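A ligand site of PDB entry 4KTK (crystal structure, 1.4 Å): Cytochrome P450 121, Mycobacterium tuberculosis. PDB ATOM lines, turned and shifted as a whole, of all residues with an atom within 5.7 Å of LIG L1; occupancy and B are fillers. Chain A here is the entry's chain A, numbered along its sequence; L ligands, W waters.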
ATOM      1  N   THR A  76       9.029 -19.413  19.392  1.00  0.00           N
ATOM      2  CA  THR A  76       9.570 -18.891  18.176  1.00  0.00           C
ATOM      3  C   THR A  76      10.510 -17.661  18.415  1.00  0.00           C
ATOM      4  O   THR A  76      11.049 -17.105  17.470  1.00  0.00           O
ATOM      5  CB  THR A  76       8.525 -18.483  17.159  1.00  0.00           C
ATOM      6  OG1 THR A  76       7.746 -17.482  17.654  1.00  0.00           O
ATOM      7  CG2 THR A  76       7.559 -19.660  16.829  1.00  0.00           C
ATOM      8  N   VAL A  77      10.585 -17.214  19.673  1.00  0.00           N
ATOM      9  CA  VAL A  77      11.423 -16.077  20.123  1.00  0.00           C
ATOM     10  C   VAL A  77      12.335 -16.605  21.168  1.00  0.00           C
ATOM     11  O   VAL A  77      12.099 -17.652  21.816  1.00  0.00           O
ATOM     12  CB  VAL A  77      10.570 -14.947  20.672  1.00  0.00           C
ATOM     13  CG1 VAL A  77       9.648 -14.381  19.633  1.00  0.00           C
ATOM     14  CG2 VAL A  77       9.701 -15.337  21.887  1.00  0.00           C
ATOM     15  N   VAL A  81      12.187 -12.949  25.747  1.00  0.00           N
ATOM     16  CA  VAL A  81      11.214 -12.135  25.062  1.00  0.00           C
ATOM     17  C   VAL A  81       9.773 -12.467  25.441  1.00  0.00           C
ATOM     18  O   VAL A  81       8.899 -11.703  25.217  1.00  0.00           O
ATOM     19  CB  VAL A  81      11.464 -12.262  23.537  1.00  0.00           C
ATOM     20  CG1 VAL A  81      10.437 -11.556  22.685  1.00  0.00           C
ATOM     21  CG2 VAL A  81      12.849 -11.816  23.151  1.00  0.00           C
ATOM     22  N   VAL A  82       9.517 -13.642  26.018  1.00  0.00           N
ATOM     23  CA  VAL A  82       8.156 -13.916  26.525  1.00  0.00           C
ATOM     24  C   VAL A  82       7.825 -12.908  27.680  1.00  0.00           C
ATOM     25  O   VAL A  82       6.627 -12.631  27.945  1.00  0.00           O
ATOM     26  CB  VAL A  82       8.112 -15.346  27.000  1.00  0.00           C
ATOM     27  CG1 VAL A  82       6.769 -15.635  27.677  1.00  0.00           C
ATOM     28  CG2 VAL A  82       8.281 -16.314  25.823  1.00  0.00           C
ATOM     29  N   ASN A  84       8.588  -9.734  27.483  1.00  0.00           N
ATOM     30  CA  ASN A  84       8.938  -8.490  26.705  1.00  0.00           C
ATOM     31  C   ASN A  84       8.395  -7.315  27.408  1.00  0.00           C
ATOM     32  O   ASN A  84       9.144  -6.327  27.699  1.00  0.00           O
ATOM     33  CB  ASN A  84       8.440  -8.649  25.262  1.00  0.00           C
ATOM     34  CG  ASN A  84       8.927  -7.551  24.311  1.00  0.00           C
ATOM     35  OD1 ASN A  84      10.104  -7.120  24.368  1.00  0.00           O
ATOM     36  ND2 ASN A  84       8.030  -7.156  23.444  1.00  0.00           N
ATOM     37  N   MET A  85       7.157  -7.305  27.831  1.00  0.00           N
ATOM     38  CA  MET A  85       6.596  -6.087  28.563  1.00  0.00           C
ATOM     39  C   MET A  85       7.221  -5.851  29.915  1.00  0.00           C
ATOM     40  O   MET A  85       7.470  -4.712  30.337  1.00  0.00           O
ATOM     41  CB  MET A  85       5.081  -6.127  28.614  1.00  0.00           C
ATOM     42  CG  MET A  85       4.474  -5.602  27.284  1.00  0.00           C
ATOM     43  SD  MET A  85       4.728  -3.946  26.581  1.00  0.00           S
ATOM     44  CE  MET A  85       4.958  -2.887  28.003  1.00  0.00           C
ATOM     45  N   SER A 162       8.389 -12.349   7.287  1.00  0.00           N
ATOM     46  CA  SER A 162       8.735 -13.219   8.402  1.00  0.00           C
ATOM     47  C   SER A 162       7.475 -13.737   9.123  1.00  0.00           C
ATOM     48  O   SER A 162       7.617 -14.756   9.869  1.00  0.00           O
ATOM     49  CB  SER A 162       9.527 -12.449   9.437  1.00  0.00           C
ATOM     50  OG  SER A 162      10.792 -12.018   8.917  1.00  0.00           O
ATOM     51  N   LEU A 163       6.326 -13.108   9.002  1.00  0.00           N
ATOM     52  CA  LEU A 163       5.227 -13.383   9.916  1.00  0.00           C
ATOM     53  C   LEU A 163       4.468 -14.704   9.783  1.00  0.00           C
ATOM     54  O   LEU A 163       4.002 -15.234  10.795  1.00  0.00           O
ATOM     55  CB  LEU A 163       4.295 -12.219  10.000  1.00  0.00           C
ATOM     56  CG  LEU A 163       5.003 -10.866  10.412  1.00  0.00           C
ATOM     57  CD1 LEU A 163       3.936  -9.778  10.453  1.00  0.00           C
ATOM     58  CD2 LEU A 163       5.792 -10.897  11.669  1.00  0.00           C
ATOM     59  N   ALA A 166       6.830 -16.656  11.994  1.00  0.00           N
ATOM     60  CA  ALA A 166       7.019 -16.231  13.352  1.00  0.00           C
ATOM     61  C   ALA A 166       5.874 -16.467  14.223  1.00  0.00           C
ATOM     62  O   ALA A 166       6.056 -16.662  15.425  1.00  0.00           O
ATOM     63  CB  ALA A 166       7.304 -14.745  13.286  1.00  0.00           C
ATOM     64  N   PHE A 167       4.672 -16.381  13.688  1.00  0.00           N
ATOM     65  CA  PHE A 167       3.462 -16.616  14.412  1.00  0.00           C
ATOM     66  C   PHE A 167       2.876 -17.993  14.293  1.00  0.00           C
ATOM     67  O   PHE A 167       1.748 -18.268  14.648  1.00  0.00           O
ATOM     68  CB  PHE A 167       2.461 -15.469  14.209  1.00  0.00           C
ATOM     69  CG  PHE A 167       2.831 -14.227  14.974  1.00  0.00           C
ATOM     70  CD1 PHE A 167       2.457 -14.096  16.310  1.00  0.00           C
ATOM     71  CD2 PHE A 167       3.642 -13.280  14.416  1.00  0.00           C
ATOM     72  CE1 PHE A 167       2.849 -12.917  16.985  1.00  0.00           C
ATOM     73  CE2 PHE A 167       4.089 -12.149  15.253  1.00  0.00           C
ATOM     74  CZ  PHE A 167       3.623 -12.091  16.472  1.00  0.00           C
ATOM     75  N   MET A 168       3.679 -18.944  13.841  1.00  0.00           N
ATOM     76  CA  MET A 168       3.280 -20.346  13.932  1.00  0.00           C
ATOM     77  C   MET A 168       3.048 -20.795  15.372  1.00  0.00           C
ATOM     78  O   MET A 168       3.675 -20.253  16.302  1.00  0.00           O
ATOM     79  CB  MET A 168       4.320 -21.255  13.263  1.00  0.00           C
ATOM     80  CG  MET A 168       4.116 -21.268  11.740  1.00  0.00           C
ATOM     81  SD  MET A 168       5.465 -22.194  10.927  1.00  0.00           S
ATOM     82  CE  MET A 168       4.903 -22.138   9.192  1.00  0.00           C
ATOM     83  N   TRP A 181      14.296 -14.149  12.675  1.00  0.00           N
ATOM     84  CA  TRP A 181      14.475 -13.307  13.904  1.00  0.00           C
ATOM     85  C   TRP A 181      15.795 -12.583  13.855  1.00  0.00           C
ATOM     86  O   TRP A 181      15.877 -11.347  14.099  1.00  0.00           O
ATOM     87  CB  TRP A 181      14.436 -14.206  15.087  1.00  0.00           C
ATOM     88  CG  TRP A 181      14.607 -13.483  16.446  1.00  0.00           C
ATOM     89  CD1 TRP A 181      15.777 -13.336  17.087  1.00  0.00           C
ATOM     90  CD2 TRP A 181      13.639 -12.702  17.105  1.00  0.00           C
ATOM     91  NE1 TRP A 181      15.560 -12.664  18.229  1.00  0.00           N
ATOM     92  CE2 TRP A 181      14.252 -12.226  18.268  1.00  0.00           C
ATOM     93  CE3 TRP A 181      12.288 -12.417  16.896  1.00  0.00           C
ATOM     94  CZ2 TRP A 181      13.551 -11.405  19.225  1.00  0.00           C
ATOM     95  CZ3 TRP A 181      11.581 -11.635  17.832  1.00  0.00           C
ATOM     96  CH2 TRP A 181      12.226 -11.106  18.975  1.00  0.00           C
ATOM     97  N   ASP A 184      15.829  -9.817  11.276  1.00  0.00           N
ATOM     98  CA  ASP A 184      14.959  -8.703  11.658  1.00  0.00           C
ATOM     99  C   ASP A 184      15.564  -7.880  12.794  1.00  0.00           C
ATOM    100  O   ASP A 184      15.434  -6.639  12.796  1.00  0.00           O
ATOM    101  CB  ASP A 184      13.555  -9.190  11.908  1.00  0.00           C
ATOM    102  CG  ASP A 184      12.917  -9.777  10.690  1.00  0.00           C
ATOM    103  OD1 ASP A 184      13.316  -9.549   9.537  1.00  0.00           O
ATOM    104  OD2 ASP A 184      11.802 -10.416  10.882  1.00  0.00           O
ATOM    105  N   VAL A 227      11.160  -5.118  16.644  1.00  0.00           N
ATOM    106  CA  VAL A 227      10.747  -6.396  15.968  1.00  0.00           C
ATOM    107  C   VAL A 227       9.417  -6.830  16.540  1.00  0.00           C
ATOM    108  O   VAL A 227       8.530  -7.190  15.709  1.00  0.00           O
ATOM    109  CB  VAL A 227      11.880  -7.454  16.074  1.00  0.00           C
ATOM    110  CG1 VAL A 227      11.313  -8.755  15.557  1.00  0.00           C
ATOM    111  CG2 VAL A 227      13.121  -7.076  15.294  1.00  0.00           C
ATOM    112  N   THR A 228       9.307  -6.925  17.849  1.00  0.00           N
ATOM    113  CA  THR A 228       8.096  -7.469  18.492  1.00  0.00           C
ATOM    114  C   THR A 228       6.899  -6.629  18.236  1.00  0.00           C
ATOM    115  O   THR A 228       5.763  -7.114  18.067  1.00  0.00           O
ATOM    116  CB  THR A 228       8.323  -7.829  19.915  1.00  0.00           C
ATOM    117  OG1 THR A 228       8.694  -6.624  20.652  1.00  0.00           O
ATOM    118  CG2 THR A 228       9.320  -8.865  20.072  1.00  0.00           C
ATOM    119  N   PHE A 229       7.002  -5.297  18.381  1.00  0.00           N
ATOM    120  CA  PHE A 229       5.808  -4.442  18.221  1.00  0.00           C
ATOM    121  C   PHE A 229       5.403  -4.406  16.742  1.00  0.00           C
ATOM    122  O   PHE A 229       4.170  -4.476  16.519  1.00  0.00           O
ATOM    123  CB  PHE A 229       6.064  -2.991  18.833  1.00  0.00           C
ATOM    124  CG  PHE A 229       5.812  -2.950  20.307  1.00  0.00           C
ATOM    125  CD1 PHE A 229       6.569  -3.741  21.226  1.00  0.00           C
ATOM    126  CD2 PHE A 229       4.635  -2.387  20.807  1.00  0.00           C
ATOM    127  CE1 PHE A 229       6.267  -3.732  22.582  1.00  0.00           C
ATOM    128  CE2 PHE A 229       4.347  -2.377  22.176  1.00  0.00           C
ATOM    129  CZ  PHE A 229       5.148  -3.079  23.060  1.00  0.00           C
ATOM    130  N   GLY A 231       5.766  -7.006  14.690  1.00  0.00           N
ATOM    131  CA  GLY A 231       5.153  -8.300  14.306  1.00  0.00           C
ATOM    132  C   GLY A 231       3.846  -8.490  15.055  1.00  0.00           C
ATOM    133  O   GLY A 231       2.827  -8.942  14.450  1.00  0.00           O
ATOM    134  N   ALA A 232       3.800  -8.243  16.348  1.00  0.00           N
ATOM    135  CA  ALA A 232       2.533  -8.385  17.055  1.00  0.00           C
ATOM    136  C   ALA A 232       1.398  -7.500  16.575  1.00  0.00           C
ATOM    137  O   ALA A 232       0.297  -7.917  16.366  1.00  0.00           O
ATOM    138  CB  ALA A 232       2.670  -8.207  18.566  1.00  0.00           C
ATOM    139  N   GLN A 384      -0.861 -19.038  15.305  1.00  0.00           N
ATOM    140  CA  GLN A 384      -1.328 -18.383  16.505  1.00  0.00           C
ATOM    141  C   GLN A 384      -2.586 -17.534  16.239  1.00  0.00           C
ATOM    142  O   GLN A 384      -3.172 -17.051  17.198  1.00  0.00           O
ATOM    143  CB  GLN A 384      -0.237 -17.523  17.141  1.00  0.00           C
ATOM    144  CG  GLN A 384       0.954 -18.339  17.717  1.00  0.00           C
ATOM    145  CD  GLN A 384       2.061 -17.486  18.179  1.00  0.00           C
ATOM    146  OE1 GLN A 384       3.280 -17.730  17.876  1.00  0.00           O
ATOM    147  NE2 GLN A 384       1.745 -16.509  18.947  1.00  0.00           N
HETATM  148  C1  LIG L   1       5.279 -10.934  20.067  1.00  0.00           C
HETATM  149  C2  LIG L   1       5.264  -9.942  21.027  1.00  0.00           C
HETATM  150  C3  LIG L   1       5.835 -10.129  22.229  1.00  0.00           C
HETATM  151  O1  LIG L   1       5.766  -9.185  23.205  1.00  0.00           O
HETATM  152  C4  LIG L   1       6.321 -11.372  22.580  1.00  0.00           C
HETATM  153  C5  LIG L   1       6.227 -12.394  21.590  1.00  0.00           C
HETATM  154  C6  LIG L   1       5.748 -12.170  20.304  1.00  0.00           C
HETATM  155  C7  LIG L   1       5.626 -13.227  19.417  1.00  0.00           C
HETATM  156  C8  LIG L   1       4.854 -14.403  19.677  1.00  0.00           C
HETATM  157  N1  LIG L   1       3.942 -14.641  20.683  1.00  0.00           N
HETATM  158  N2  LIG L   1       5.005 -15.355  18.733  1.00  0.00           N
HETATM  159  N3  LIG L   1       5.862 -14.788  17.849  1.00  0.00           N
HETATM  160  C9  LIG L   1       6.245 -13.509  18.254  1.00  0.00           C
HETATM  161  C10 LIG L   1       7.131 -12.816  17.406  1.00  0.00           C
HETATM  162  C11 LIG L   1       6.995 -11.391  17.131  1.00  0.00           C
HETATM  163  C12 LIG L   1       7.763 -10.785  16.150  1.00  0.00           C
HETATM  164  C13 LIG L   1       8.643 -11.535  15.377  1.00  0.00           C
HETATM  165  O2  LIG L   1       9.367 -10.988  14.374  1.00  0.00           O
HETATM  166  C14 LIG L   1       8.856 -12.856  15.696  1.00  0.00           C
HETATM  167  C15 LIG L   1       8.014 -13.486  16.540  1.00  0.00           C
HETATM  168  O3  LIG L   1       8.301 -14.874  16.686  1.00  0.00           O
HETATM  169  C1  LG2 L   2      -0.909  -8.528  23.989  1.00  0.00           C
HETATM  170  C2  LG2 L   2      -4.896  -8.816  21.285  1.00  0.00           C
HETATM  171  C3  LG2 L   2      -3.137  -5.192  18.492  1.00  0.00           C
HETATM  172  C4  LG2 L   2       1.076  -5.497  20.785  1.00  0.00           C
HETATM  173  C5  LG2 L   2      -2.200  -8.843  23.597  1.00  0.00           C
HETATM  174  C6  LG2 L   2      -3.108  -9.778  24.197  1.00  0.00           C
HETATM  175  C7  LG2 L   2      -4.192  -9.918  23.453  1.00  0.00           C
HETATM  176  C8  LG2 L   2      -3.997  -9.036  22.283  1.00  0.00           C
HETATM  177  C9  LG2 L   2      -5.389 -10.734  23.596  1.00  0.00           C
HETATM  178  C10 LG2 L   2      -2.855 -10.403  25.566  1.00  0.00           C
HETATM  179  C11 LG2 L   2      -2.035 -11.646  25.545  1.00  0.00           C
HETATM  180  C12 LG2 L   2      -1.870 -12.301  26.848  1.00  0.00           C
HETATM  181  O1  LG2 L   2      -2.317 -11.793  27.907  1.00  0.00           O
HETATM  182  O2  LG2 L   2      -1.307 -13.442  26.911  1.00  0.00           O
HETATM  183  C13 LG2 L   2      -4.781  -7.869  20.223  1.00  0.00           C
HETATM  184  C14 LG2 L   2      -5.755  -7.607  19.242  1.00  0.00           C
HETATM  185  C15 LG2 L   2      -5.290  -6.578  18.417  1.00  0.00           C
HETATM  186  C16 LG2 L   2      -3.970  -6.199  18.948  1.00  0.00           C
HETATM  187  C17 LG2 L   2      -7.041  -8.287  19.096  1.00  0.00           C
HETATM  188  C18 LG2 L   2      -5.925  -5.870  17.306  1.00  0.00           C
HETATM  189  C19 LG2 L   2      -7.176  -5.861  17.083  1.00  0.00           C
HETATM  190  C20 LG2 L   2      -1.859  -4.854  18.910  1.00  0.00           C
HETATM  191  C21 LG2 L   2      -1.031  -3.822  18.359  1.00  0.00           C
HETATM  192  C22 LG2 L   2       0.132  -3.988  18.997  1.00  0.00           C
HETATM  193  C23 LG2 L   2       0.086  -5.073  19.926  1.00  0.00           C
HETATM  194  C24 LG2 L   2      -1.548  -2.815  17.367  1.00  0.00           C
HETATM  195  C25 LG2 L   2       1.329  -3.143  18.808  1.00  0.00           C
HETATM  196  C26 LG2 L   2       1.595  -2.220  17.851  1.00  0.00           C
HETATM  197  C27 LG2 L   2       0.950  -6.426  21.786  1.00  0.00           C
HETATM  198  C28 LG2 L   2       1.997  -6.842  22.730  1.00  0.00           C
HETATM  199  C29 LG2 L   2       1.400  -7.652  23.677  1.00  0.00           C
HETATM  200  C30 LG2 L   2       0.026  -7.798  23.288  1.00  0.00           C
HETATM  201  C31 LG2 L   2       3.401  -6.327  22.679  1.00  0.00           C
HETATM  202  C32 LG2 L   2       2.092  -8.325  24.842  1.00  0.00           C
HETATM  203  C33 LG2 L   2       1.817  -7.623  26.143  1.00  0.00           C
HETATM  204  C34 LG2 L   2       2.384  -8.286  27.436  1.00  0.00           C
HETATM  205  O3  LG2 L   2       2.134  -7.689  28.488  1.00  0.00           O
HETATM  206  O4  LG2 L   2       3.124  -9.218  27.320  1.00  0.00           O
HETATM  207  N1  LG2 L   2      -2.752  -8.397  22.431  1.00  0.00           N
HETATM  208  N2  LG2 L   2      -3.755  -7.004  20.051  1.00  0.00           N
HETATM  209  N3  LG2 L   2      -1.246  -5.557  19.901  1.00  0.00           N
HETATM  210  N4  LG2 L   2      -0.284  -6.960  22.223  1.00  0.00           N
HETATM  211 FE1  LG2 L   2      -2.028  -6.914  21.214  1.00  0.00          FE
HETATM  212  O   HOH W   1      11.268 -12.283  12.917  1.00  0.00           O
HETATM  213  O   HOH W   2       5.860 -16.339  22.473  1.00  0.00           O
HETATM  214  O   HOH W   3       8.248  -8.708  13.349  1.00  0.00           O
HETATM  215  O   HOH W   4       5.241 -10.186  25.595  1.00  0.00           O
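An oxygen (O3) of LIG L1 lies within hydrogen-bond range of the side-chain hydroxyl (OG1) of Thr 76, at 2.8 Å. The side-chain amide oxygen (OE1) of Gln 384 lies close to a nitrogen (N2) of LIG L1 (3.1 Å). N3 of LIG L1 sits at hydrogen-bond distance from O of Ala 166. The side-chain amide nitrogen (ND2) of Asn 84 lies within hydrogen-bond range of an oxygen (O1) of LIG L1, at 3.0 Å.
The side-chain amide oxygen (OE1) of Gln 384 sits close to the backbone carbonyl oxygen (O) of Met 168, at 3.0 Å. The backbone carbonyl oxygen (O) of Ala 166 sits at hydrogen-bond distance from the side-chain hydroxyl (OG1) of Thr 76 (2.9 Å). The backbone NH (N) of Gln 384 lies within hydrogen-bond range of the backbone carbonyl oxygen (O) of Phe 167, at 2.8 Å. OG1 of Thr 228 lies within hydrogen-bond range of ND2 of Asn 84 (2.9 Å).
Residues that only touch LIG L1: Val 227 (3.2 Å), Val 77 (3.3 Å), Phe 167 (3.5 Å), Trp 181 (3.7 Å), Val 81 (3.7 Å), Thr 228 (3.9 Å) and Ala 232 (3.97 Å).
Water W4 bridges O1 of LIG L1 (2.6 Å) and O4 of LG2 L2 (2.9 Å). Water W1 bridges an oxygen (O2) of LIG L1 (2.7 Å) and the side-chain carboxylate (OD2) of Asp 184 (2.8 Å). Water W3 lies within hydrogen-bond range of an oxygen (O2) of LIG L1 (2.7 Å), the backbone carbonyl oxygen of Val 227 (2.8 Å) and the backbone NH of Gly 231 (3.3 Å).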
